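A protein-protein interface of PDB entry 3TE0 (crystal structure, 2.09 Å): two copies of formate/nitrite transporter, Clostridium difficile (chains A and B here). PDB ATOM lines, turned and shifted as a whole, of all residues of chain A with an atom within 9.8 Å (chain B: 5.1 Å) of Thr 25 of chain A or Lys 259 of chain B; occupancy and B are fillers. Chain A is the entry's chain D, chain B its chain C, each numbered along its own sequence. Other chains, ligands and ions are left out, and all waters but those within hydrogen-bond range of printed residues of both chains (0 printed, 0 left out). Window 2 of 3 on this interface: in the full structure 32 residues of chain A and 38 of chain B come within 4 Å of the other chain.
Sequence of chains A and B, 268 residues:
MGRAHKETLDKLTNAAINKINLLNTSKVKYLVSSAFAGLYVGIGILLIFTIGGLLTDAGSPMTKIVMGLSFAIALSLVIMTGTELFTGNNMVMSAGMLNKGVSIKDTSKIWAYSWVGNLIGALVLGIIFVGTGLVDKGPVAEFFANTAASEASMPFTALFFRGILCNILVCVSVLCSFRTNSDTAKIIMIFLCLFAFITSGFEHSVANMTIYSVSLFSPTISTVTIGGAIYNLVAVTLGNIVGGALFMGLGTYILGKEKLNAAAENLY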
ATOM      1  N   ILE A  17     -33.817  26.522  14.828  1.00  0.00           N
ATOM      2  CA  ILE A  17     -33.022  26.681  13.603  1.00  0.00           C
ATOM      3  C   ILE A  17     -31.736  25.858  13.734  1.00  0.00           C
ATOM      4  O   ILE A  17     -31.361  25.130  12.814  1.00  0.00           O
ATOM      5  CB  ILE A  17     -32.715  28.162  13.329  1.00  0.00           C
ATOM      6  CG1 ILE A  17     -34.006  28.907  12.967  1.00  0.00           C
ATOM      7  CG2 ILE A  17     -31.638  28.341  12.196  1.00  0.00           C
ATOM      8  CD1 ILE A  17     -33.823  30.423  12.824  1.00  0.00           C
ATOM      9  N   ASN A  18     -31.091  25.961  14.896  1.00  0.00           N
ATOM     10  CA  ASN A  18     -29.886  25.193  15.201  1.00  0.00           C
ATOM     11  C   ASN A  18     -30.089  23.673  15.120  1.00  0.00           C
ATOM     12  O   ASN A  18     -29.236  22.951  14.596  1.00  0.00           O
ATOM     13  CB  ASN A  18     -29.352  25.583  16.582  1.00  0.00           C
ATOM     14  CG  ASN A  18     -28.646  26.925  16.565  1.00  0.00           C
ATOM     15  OD1 ASN A  18     -28.268  27.420  15.504  1.00  0.00           O
ATOM     16  ND2 ASN A  18     -28.467  27.523  17.736  1.00  0.00           N
ATOM     17  N   LYS A  19     -31.221  23.197  15.630  1.00  0.00           N
ATOM     18  CA  LYS A  19     -31.536  21.768  15.561  1.00  0.00           C
ATOM     19  C   LYS A  19     -31.654  21.231  14.128  1.00  0.00           C
ATOM     20  O   LYS A  19     -31.043  20.219  13.782  1.00  0.00           O
ATOM     21  CB  LYS A  19     -32.802  21.458  16.359  1.00  0.00           C
ATOM     22  CG  LYS A  19     -32.638  21.662  17.861  1.00  0.00           C
ATOM     23  CD  LYS A  19     -33.963  21.483  18.598  1.00  0.00           C
ATOM     24  CE  LYS A  19     -33.802  21.795  20.081  1.00  0.00           C
ATOM     25  NZ  LYS A  19     -33.215  20.666  20.838  1.00  0.00           N
ATOM     26  N   ILE A  20     -32.445  21.903  13.299  1.00  0.00           N
ATOM     27  CA  ILE A  20     -32.615  21.462  11.923  1.00  0.00           C
ATOM     28  C   ILE A  20     -31.324  21.638  11.113  1.00  0.00           C
ATOM     29  O   ILE A  20     -31.036  20.827  10.239  1.00  0.00           O
ATOM     30  CB  ILE A  20     -33.822  22.139  11.220  1.00  0.00           C
ATOM     31  CG1 ILE A  20     -34.043  21.538   9.819  1.00  0.00           C
ATOM     32  CG2 ILE A  20     -33.643  23.661  11.152  1.00  0.00           C
ATOM     33  CD1 ILE A  20     -34.346  20.047   9.820  1.00  0.00           C
ATOM     34  N   ASN A  21     -30.541  22.679  11.407  1.00  0.00           N
ATOM     35  CA  ASN A  21     -29.257  22.842  10.722  1.00  0.00           C
ATOM     36  C   ASN A  21     -28.295  21.712  11.097  1.00  0.00           C
ATOM     37  O   ASN A  21     -27.517  21.246  10.266  1.00  0.00           O
ATOM     38  CB  ASN A  21     -28.615  24.207  11.017  1.00  0.00           C
ATOM     39  CG  ASN A  21     -29.339  25.363  10.344  1.00  0.00           C
ATOM     40  OD1 ASN A  21     -30.143  25.168   9.440  1.00  0.00           O
ATOM     41  ND2 ASN A  21     -29.038  26.576  10.773  1.00  0.00           N
ATOM     42  N   LEU A  22     -28.342  21.291  12.358  1.00  0.00           N
ATOM     43  CA  LEU A  22     -27.510  20.187  12.833  1.00  0.00           C
ATOM     44  C   LEU A  22     -27.865  18.895  12.093  1.00  0.00           C
ATOM     45  O   LEU A  22     -26.991  18.209  11.546  1.00  0.00           O
ATOM     46  CB  LEU A  22     -27.675  19.991  14.345  1.00  0.00           C
ATOM     47  CG  LEU A  22     -26.880  18.836  14.963  1.00  0.00           C
ATOM     48  CD1 LEU A  22     -25.385  18.980  14.671  1.00  0.00           C
ATOM     49  CD2 LEU A  22     -27.138  18.753  16.460  1.00  0.00           C
ATOM     50  N   LEU A  23     -29.157  18.583  12.068  1.00  0.00           N
ATOM     51  CA  LEU A  23     -29.641  17.387  11.409  1.00  0.00           C
ATOM     52  C   LEU A  23     -29.270  17.377   9.935  1.00  0.00           C
ATOM     53  O   LEU A  23     -28.853  16.346   9.423  1.00  0.00           O
ATOM     54  CB  LEU A  23     -31.161  17.247  11.560  1.00  0.00           C
ATOM     55  CG  LEU A  23     -31.758  16.041  10.820  1.00  0.00           C
ATOM     56  CD1 LEU A  23     -31.089  14.743  11.282  1.00  0.00           C
ATOM     57  CD2 LEU A  23     -33.278  15.970  10.993  1.00  0.00           C
ATOM     58  N   ASN A  24     -29.441  18.517   9.258  1.00  0.00           N
ATOM     59  CA  ASN A  24     -29.085  18.639   7.842  1.00  0.00           C
ATOM     60  C   ASN A  24     -27.589  18.504   7.613  1.00  0.00           C
ATOM     61  O   ASN A  24     -27.151  18.120   6.537  1.00  0.00           O
ATOM     62  CB  ASN A  24     -29.544  19.983   7.263  1.00  0.00           C
ATOM     63  CG  ASN A  24     -31.048  20.066   7.095  1.00  0.00           C
ATOM     64  OD1 ASN A  24     -31.743  19.047   7.113  1.00  0.00           O
ATOM     65  ND2 ASN A  24     -31.556  21.285   6.909  1.00  0.00           N
ATOM     66  N   THR A  25     -26.809  18.846   8.628  1.00  0.00           N
ATOM     67  CA  THR A  25     -25.361  18.832   8.500  1.00  0.00           C
ATOM     68  C   THR A  25     -24.855  17.413   8.698  1.00  0.00           C
ATOM     69  O   THR A  25     -23.966  16.961   7.978  1.00  0.00           O
ATOM     70  CB  THR A  25     -24.695  19.762   9.544  1.00  0.00           C
ATOM     71  OG1 THR A  25     -24.988  21.126   9.218  1.00  0.00           O
ATOM     72  CG2 THR A  25     -23.179  19.561   9.567  1.00  0.00           C
ATOM     73  N   SER A  26     -25.428  16.721   9.683  1.00  0.00           N
ATOM     74  CA  SER A  26     -25.012  15.366   9.997  1.00  0.00           C
ATOM     75  C   SER A  26     -26.074  14.561  10.736  1.00  0.00           C
ATOM     76  O   SER A  26     -26.416  14.854  11.896  1.00  0.00           O
ATOM     77  CB  SER A  26     -23.723  15.373  10.810  1.00  0.00           C
ATOM     78  OG  SER A  26     -23.413  14.061  11.240  1.00  0.00           O
ATOM     79  N   LYS A  27     -26.589  13.535  10.064  1.00  0.00           N
ATOM     80  CA  LYS A  27     -27.549  12.632  10.689  1.00  0.00           C
ATOM     81  C   LYS A  27     -26.865  11.855  11.794  1.00  0.00           C
ATOM     82  O   LYS A  27     -27.486  11.499  12.788  1.00  0.00           O
ATOM     83  CB  LYS A  27     -28.132  11.665   9.659  1.00  0.00           C
ATOM     84  CG  LYS A  27     -29.059  12.301   8.642  1.00  0.00           C
ATOM     85  CD  LYS A  27     -29.518  11.256   7.643  1.00  0.00           C
ATOM     86  CE  LYS A  27     -30.461  11.836   6.600  1.00  0.00           C
ATOM     87  NZ  LYS A  27     -29.736  12.720   5.645  1.00  0.00           N
ATOM     88  N   VAL A  28     -25.573  11.597  11.634  1.00  0.00           N
ATOM     89  CA  VAL A  28     -24.850  10.853  12.655  1.00  0.00           C
ATOM     90  C   VAL A  28     -24.741  11.683  13.936  1.00  0.00           C
ATOM     91  O   VAL A  28     -25.058  11.204  15.024  1.00  0.00           O
ATOM     92  CB  VAL A  28     -23.454  10.416  12.174  1.00  0.00           C
ATOM     93  CG1 VAL A  28     -22.660   9.777  13.322  1.00  0.00           C
ATOM     94  CG2 VAL A  28     -23.573   9.476  10.970  1.00  0.00           C
ATOM     95  N   LYS A  29     -24.303  12.932  13.809  1.00  0.00           N
ATOM     96  CA  LYS A  29     -24.187  13.785  14.988  1.00  0.00           C
ATOM     97  C   LYS A  29     -25.551  13.968  15.643  1.00  0.00           C
ATOM     98  O   LYS A  29     -25.663  13.993  16.878  1.00  0.00           O
ATOM     99  CB  LYS A  29     -23.580  15.156  14.631  1.00  0.00           C
ATOM    100  CG  LYS A  29     -22.077  15.129  14.342  1.00  0.00           C
ATOM    101  CD  LYS A  29     -21.626  16.431  13.680  1.00  0.00           C
ATOM    102  CE  LYS A  29     -20.118  16.645  13.803  1.00  0.00           C
ATOM    103  NZ  LYS A  29     -19.753  17.031  15.196  1.00  0.00           N
ATOM    104  N   TYR A  30     -26.596  14.084  14.825  1.00  0.00           N
ATOM    105  CA  TYR A  30     -27.919  14.348  15.382  1.00  0.00           C
ATOM    106  C   TYR A  30     -28.457  13.130  16.138  1.00  0.00           C
ATOM    107  O   TYR A  30     -29.015  13.251  17.234  1.00  0.00           O
ATOM    108  CB  TYR A  30     -28.933  14.820  14.324  1.00  0.00           C
ATOM    109  CG  TYR A  30     -30.192  15.309  15.011  1.00  0.00           C
ATOM    110  CD1 TYR A  30     -30.283  16.622  15.469  1.00  0.00           C
ATOM    111  CD2 TYR A  30     -31.253  14.442  15.267  1.00  0.00           C
ATOM    112  CE1 TYR A  30     -31.412  17.078  16.145  1.00  0.00           C
ATOM    113  CE2 TYR A  30     -32.395  14.886  15.954  1.00  0.00           C
ATOM    114  CZ  TYR A  30     -32.465  16.200  16.388  1.00  0.00           C
ATOM    115  OH  TYR A  30     -33.583  16.650  17.063  1.00  0.00           O
ATOM    116  N   LEU A  31     -28.291  11.960  15.531  1.00  0.00           N
ATOM    117  CA  LEU A  31     -28.742  10.705  16.125  1.00  0.00           C
ATOM    118  C   LEU A  31     -27.937  10.305  17.353  1.00  0.00           C
ATOM    119  O   LEU A  31     -28.495   9.772  18.310  1.00  0.00           O
ATOM    120  CB  LEU A  31     -28.723   9.580  15.079  1.00  0.00           C
ATOM    121  CG  LEU A  31     -29.865   9.743  14.072  1.00  0.00           C
ATOM    122  CD1 LEU A  31     -29.690   8.799  12.879  1.00  0.00           C
ATOM    123  CD2 LEU A  31     -31.208   9.534  14.767  1.00  0.00           C
ATOM    124  N   LYS A 109     -39.407  16.358  10.703  1.00  0.00           N
ATOM    125  CA  LYS A 109     -38.113  15.703  10.570  1.00  0.00           C
ATOM    126  C   LYS A 109     -37.360  15.643  11.925  1.00  0.00           C
ATOM    127  O   LYS A 109     -36.893  14.588  12.343  1.00  0.00           O
ATOM    128  CB  LYS A 109     -37.283  16.439   9.523  1.00  0.00           C
ATOM    129  CG  LYS A 109     -36.483  15.544   8.603  1.00  0.00           C
ATOM    130  CD  LYS A 109     -35.801  16.367   7.519  1.00  0.00           C
ATOM    131  CE  LYS A 109     -34.663  15.596   6.866  1.00  0.00           C
ATOM    132  NZ  LYS A 109     -33.995  16.396   5.791  1.00  0.00           N
ATOM    133  N   ILE A 110     -37.248  16.778  12.603  1.00  0.00           N
ATOM    134  CA  ILE A 110     -36.644  16.807  13.943  1.00  0.00           C
ATOM    135  C   ILE A 110     -37.374  15.877  14.922  1.00  0.00           C
ATOM    136  O   ILE A 110     -36.740  15.109  15.667  1.00  0.00           O
ATOM    137  CB  ILE A 110     -36.569  18.252  14.496  1.00  0.00           C
ATOM    138  CG1 ILE A 110     -35.490  19.046  13.747  1.00  0.00           C
ATOM    139  CG2 ILE A 110     -36.314  18.274  16.038  1.00  0.00           C
ATOM    140  CD1 ILE A 110     -34.066  18.486  13.910  1.00  0.00           C
ATOM    141  N   LYS B 257     -16.619  17.199  17.108  1.00  0.00           N
ATOM    142  CA  LYS B 257     -15.666  17.364  16.021  1.00  0.00           C
ATOM    143  C   LYS B 257     -16.317  18.019  14.798  1.00  0.00           C
ATOM    144  O   LYS B 257     -17.262  17.473  14.234  1.00  0.00           O
ATOM    145  CB  LYS B 257     -15.060  16.009  15.635  1.00  0.00           C
ATOM    146  CG  LYS B 257     -13.977  16.083  14.548  1.00  0.00           C
ATOM    147  CD  LYS B 257     -12.685  16.705  15.078  1.00  0.00           C
ATOM    148  CE  LYS B 257     -11.514  16.516  14.060  1.00  0.00           C
ATOM    149  NZ  LYS B 257     -10.212  16.911  14.703  1.00  0.00           N
ATOM    150  N   GLU B 258     -15.817  19.184  14.390  1.00  0.00           N
ATOM    151  CA  GLU B 258     -16.397  19.892  13.251  1.00  0.00           C
ATOM    152  C   GLU B 258     -16.225  19.062  11.992  1.00  0.00           C
ATOM    153  O   GLU B 258     -15.128  18.570  11.718  1.00  0.00           O
ATOM    154  CB  GLU B 258     -15.759  21.277  13.070  1.00  0.00           C
ATOM    155  CG  GLU B 258     -16.246  22.320  14.069  1.00  0.00           C
ATOM    156  CD  GLU B 258     -15.889  23.748  13.667  1.00  0.00           C
ATOM    157  OE1 GLU B 258     -16.574  24.686  14.127  1.00  0.00           O
ATOM    158  OE2 GLU B 258     -14.925  23.938  12.894  1.00  0.00           O
ATOM    159  N   LYS B 259     -17.299  18.897  11.225  1.00  0.00           N
ATOM    160  CA  LYS B 259     -17.255  17.973  10.090  1.00  0.00           C
ATOM    161  C   LYS B 259     -16.264  18.348   8.972  1.00  0.00           C
ATOM    162  O   LYS B 259     -15.758  17.458   8.271  1.00  0.00           O
ATOM    163  CB  LYS B 259     -18.665  17.626   9.564  1.00  0.00           C
ATOM    164  CG  LYS B 259     -19.171  18.390   8.338  1.00  0.00           C
ATOM    165  CD  LYS B 259     -20.386  17.653   7.747  1.00  0.00           C
ATOM    166  CE  LYS B 259     -21.062  18.427   6.615  1.00  0.00           C
ATOM    167  NZ  LYS B 259     -22.007  17.576   5.820  1.00  0.00           N
ATOM    168  N   LEU B 260     -15.970  19.634   8.796  1.00  0.00           N
ATOM    169  CA  LEU B 260     -14.931  20.003   7.824  1.00  0.00           C
ATOM    170  C   LEU B 260     -13.600  19.503   8.400  1.00  0.00           C
ATOM    171  O   LEU B 260     -13.156  20.000   9.442  1.00  0.00           O
ATOM    172  CB  LEU B 260     -14.917  21.511   7.574  1.00  0.00           C
ATOM    173  CG  LEU B 260     -13.924  22.055   6.556  1.00  0.00           C
ATOM    174  CD1 LEU B 260     -14.096  21.369   5.193  1.00  0.00           C
ATOM    175  CD2 LEU B 260     -14.054  23.572   6.425  1.00  0.00           C
ATOM    176  N   ASN B 261     -12.983  18.530   7.716  1.00  0.00           N
ATOM    177  CA  ASN B 261     -12.017  17.572   8.308  1.00  0.00           C
ATOM    178  C   ASN B 261     -12.703  16.272   8.787  1.00  0.00           C
ATOM    179  O   ASN B 261     -12.796  16.027   9.999  1.00  0.00           O
ATOM    180  CB  ASN B 261     -11.265  18.159   9.503  1.00  0.00           C
ATOM    181  CG  ASN B 261     -12.155  18.326  10.662  1.00  0.00           C
ATOM    182  OD1 ASN B 261     -11.962  19.207  11.515  1.00  0.00           O
ATOM    183  ND2 ASN B 261     -13.205  17.501  10.691  1.00  0.00           N
ATOM    184  N   ALA B 262     -13.180  15.437   7.880  1.00  0.00           N
ATOM    185  CA  ALA B 262     -12.991  15.589   6.433  1.00  0.00           C
ATOM    186  C   ALA B 262     -11.513  15.775   6.086  1.00  0.00           C
ATOM    187  O   ALA B 262     -10.972  14.991   5.322  1.00  0.00           O
ATOM    188  CB  ALA B 262     -13.872  16.696   5.846  1.00  0.00           C
ATOM    189  N   GLU B 265     -11.818  12.644   7.749  1.00  0.00           N
ATOM    190  CA  GLU B 265     -12.979  11.708   7.728  1.00  0.00           C
ATOM    191  C   GLU B 265     -14.449  12.253   7.744  1.00  0.00           C
ATOM    192  O   GLU B 265     -14.715  13.368   8.177  1.00  0.00           O
ATOM    193  CB  GLU B 265     -12.826  10.703   8.870  1.00  0.00           C
ATOM    194  CG  GLU B 265     -12.758  11.354  10.228  1.00  0.00           C
ATOM    195  CD  GLU B 265     -13.996  11.078  11.053  1.00  0.00           C
ATOM    196  OE1 GLU B 265     -14.177  11.737  12.099  1.00  0.00           O
ATOM    197  OE2 GLU B 265     -14.783  10.191  10.654  1.00  0.00           O
ATOM    198  N   LEU B 267     -18.549  12.343   8.275  1.00  0.00           N
ATOM    199  CA  LEU B 267     -19.629  11.976   9.195  1.00  0.00           C
ATOM    200  C   LEU B 267     -20.941  11.573   8.510  1.00  0.00           C
ATOM    201  O   LEU B 267     -21.431  10.465   8.735  1.00  0.00           O
ATOM    202  CB  LEU B 267     -19.844  13.062  10.264  1.00  0.00           C
ATOM    203  CG  LEU B 267     -18.698  13.100  11.288  1.00  0.00           C
ATOM    204  CD1 LEU B 267     -18.095  14.492  11.477  1.00  0.00           C
ATOM    205  CD2 LEU B 267     -19.100  12.503  12.634  1.00  0.00           C
ATOM    206  N   TYR B 268     -21.490  12.448   7.669  1.00  0.00           N
ATOM    207  CA  TYR B 268     -22.816  12.225   7.066  1.00  0.00           C
ATOM    208  C   TYR B 268     -23.934  11.952   8.094  1.00  0.00           C
ATOM    209  O   TYR B 268     -25.085  12.363   7.906  1.00  0.00           O
ATOM    210  CB  TYR B 268     -22.772  11.129   5.987  1.00  0.00           C
ATOM    211  CG  TYR B 268     -22.541   9.709   6.478  1.00  0.00           C
ATOM    212  CD1 TYR B 268     -23.603   8.916   6.903  1.00  0.00           C
ATOM    213  CD2 TYR B 268     -21.264   9.149   6.479  1.00  0.00           C
ATOM    214  CE1 TYR B 268     -23.398   7.613   7.335  1.00  0.00           C
ATOM    215  CE2 TYR B 268     -21.050   7.848   6.911  1.00  0.00           C
ATOM    216  CZ  TYR B 268     -22.121   7.087   7.338  1.00  0.00           C
ATOM    217  OH  TYR B 268     -21.919   5.796   7.768  1.00  0.00           O
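The side-chain amino group (NZ) of Lys 259 of chain B is in hydrogen-bond range of the backbone carbonyl oxygen (O) of Thr 25 of chain A.
O of Lys 257 of chain B lies within hydrogen-bond range of NZ of Lys 29 of chain A (2.7 Å).
The backbone carbonyl oxygen (O) of Tyr 268 of chain B lies within hydrogen-bond range of the backbone NH (N) of Lys 27 of chain A (2.9 Å).
The backbone carbonyl oxygen (O) of Asn 21 of chain A lies within hydrogen-bond range of the side-chain hydroxyl (OG1) of Thr 25 of chain A (2.7 Å).
The backbone NH (N) of Val 28 of chain A sits close to the side-chain hydroxyl (OG) of Ser 26 of chain A, 3.3 Å away.
The backbone NH of Lys 29 of chain A is in hydrogen-bond range of the side-chain hydroxyl of Ser 26 of chain A, at 2.9 Å.
Ser 26 of chain A touches Leu 267 of chain B (OG to CB, 3.8 Å).
Tyr 268 of chain B touches Ser 26 of chain A (O to CA, 3.7 Å).
Leu 267 of chain B touches Val 28 of chain A.
Val 28 of chain A touches Tyr 268 of chain B.
CE of Lys 29 of chain A touches CD1 of Leu 267 of chain B (3.8 Å).
Thr 25 of chain A touches one residue of chain B.
Lys 259 of chain B touches just one residue of chain A: Thr 25.
No residue of chain A comes within 4 Å of Asn 261 of chain B.
Of the printed residues of chain B, Ser 26 of chain A touches Leu 267 and Tyr 268.
Of the printed residues of chain B, Val 28 of chain A touches Leu 267 (3.2 Å) and Tyr 268 (3.8 Å).
Of the printed residues of chain B, Lys 27 of chain A touches Tyr 268 (2.9 Å).
Of the printed residues of chain B, Lys 29 of chain A touches Lys 257 and Leu 267.
Ile 20 of chain A touches none of the printed residues of chain B.
The nearest printed residue of chain A that does not touch Tyr 268 of chain B is Thr 25 of chain A (4.7 Å).
Of the 17 printed residues of chain A, 5 touch a printed residue of chain B.
Hydrophobic or aromatic side chains of chain A within 4 Å of the printed part of chain B: Val 28.
Hydrophobic or aromatic side chains of chain B that line the printed part of chain A: Leu 267.
No position is printed for both chains.
Of the 8 pairs that touch across the chains among the printed residues, none has its exchanged pair printed and touching as well.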
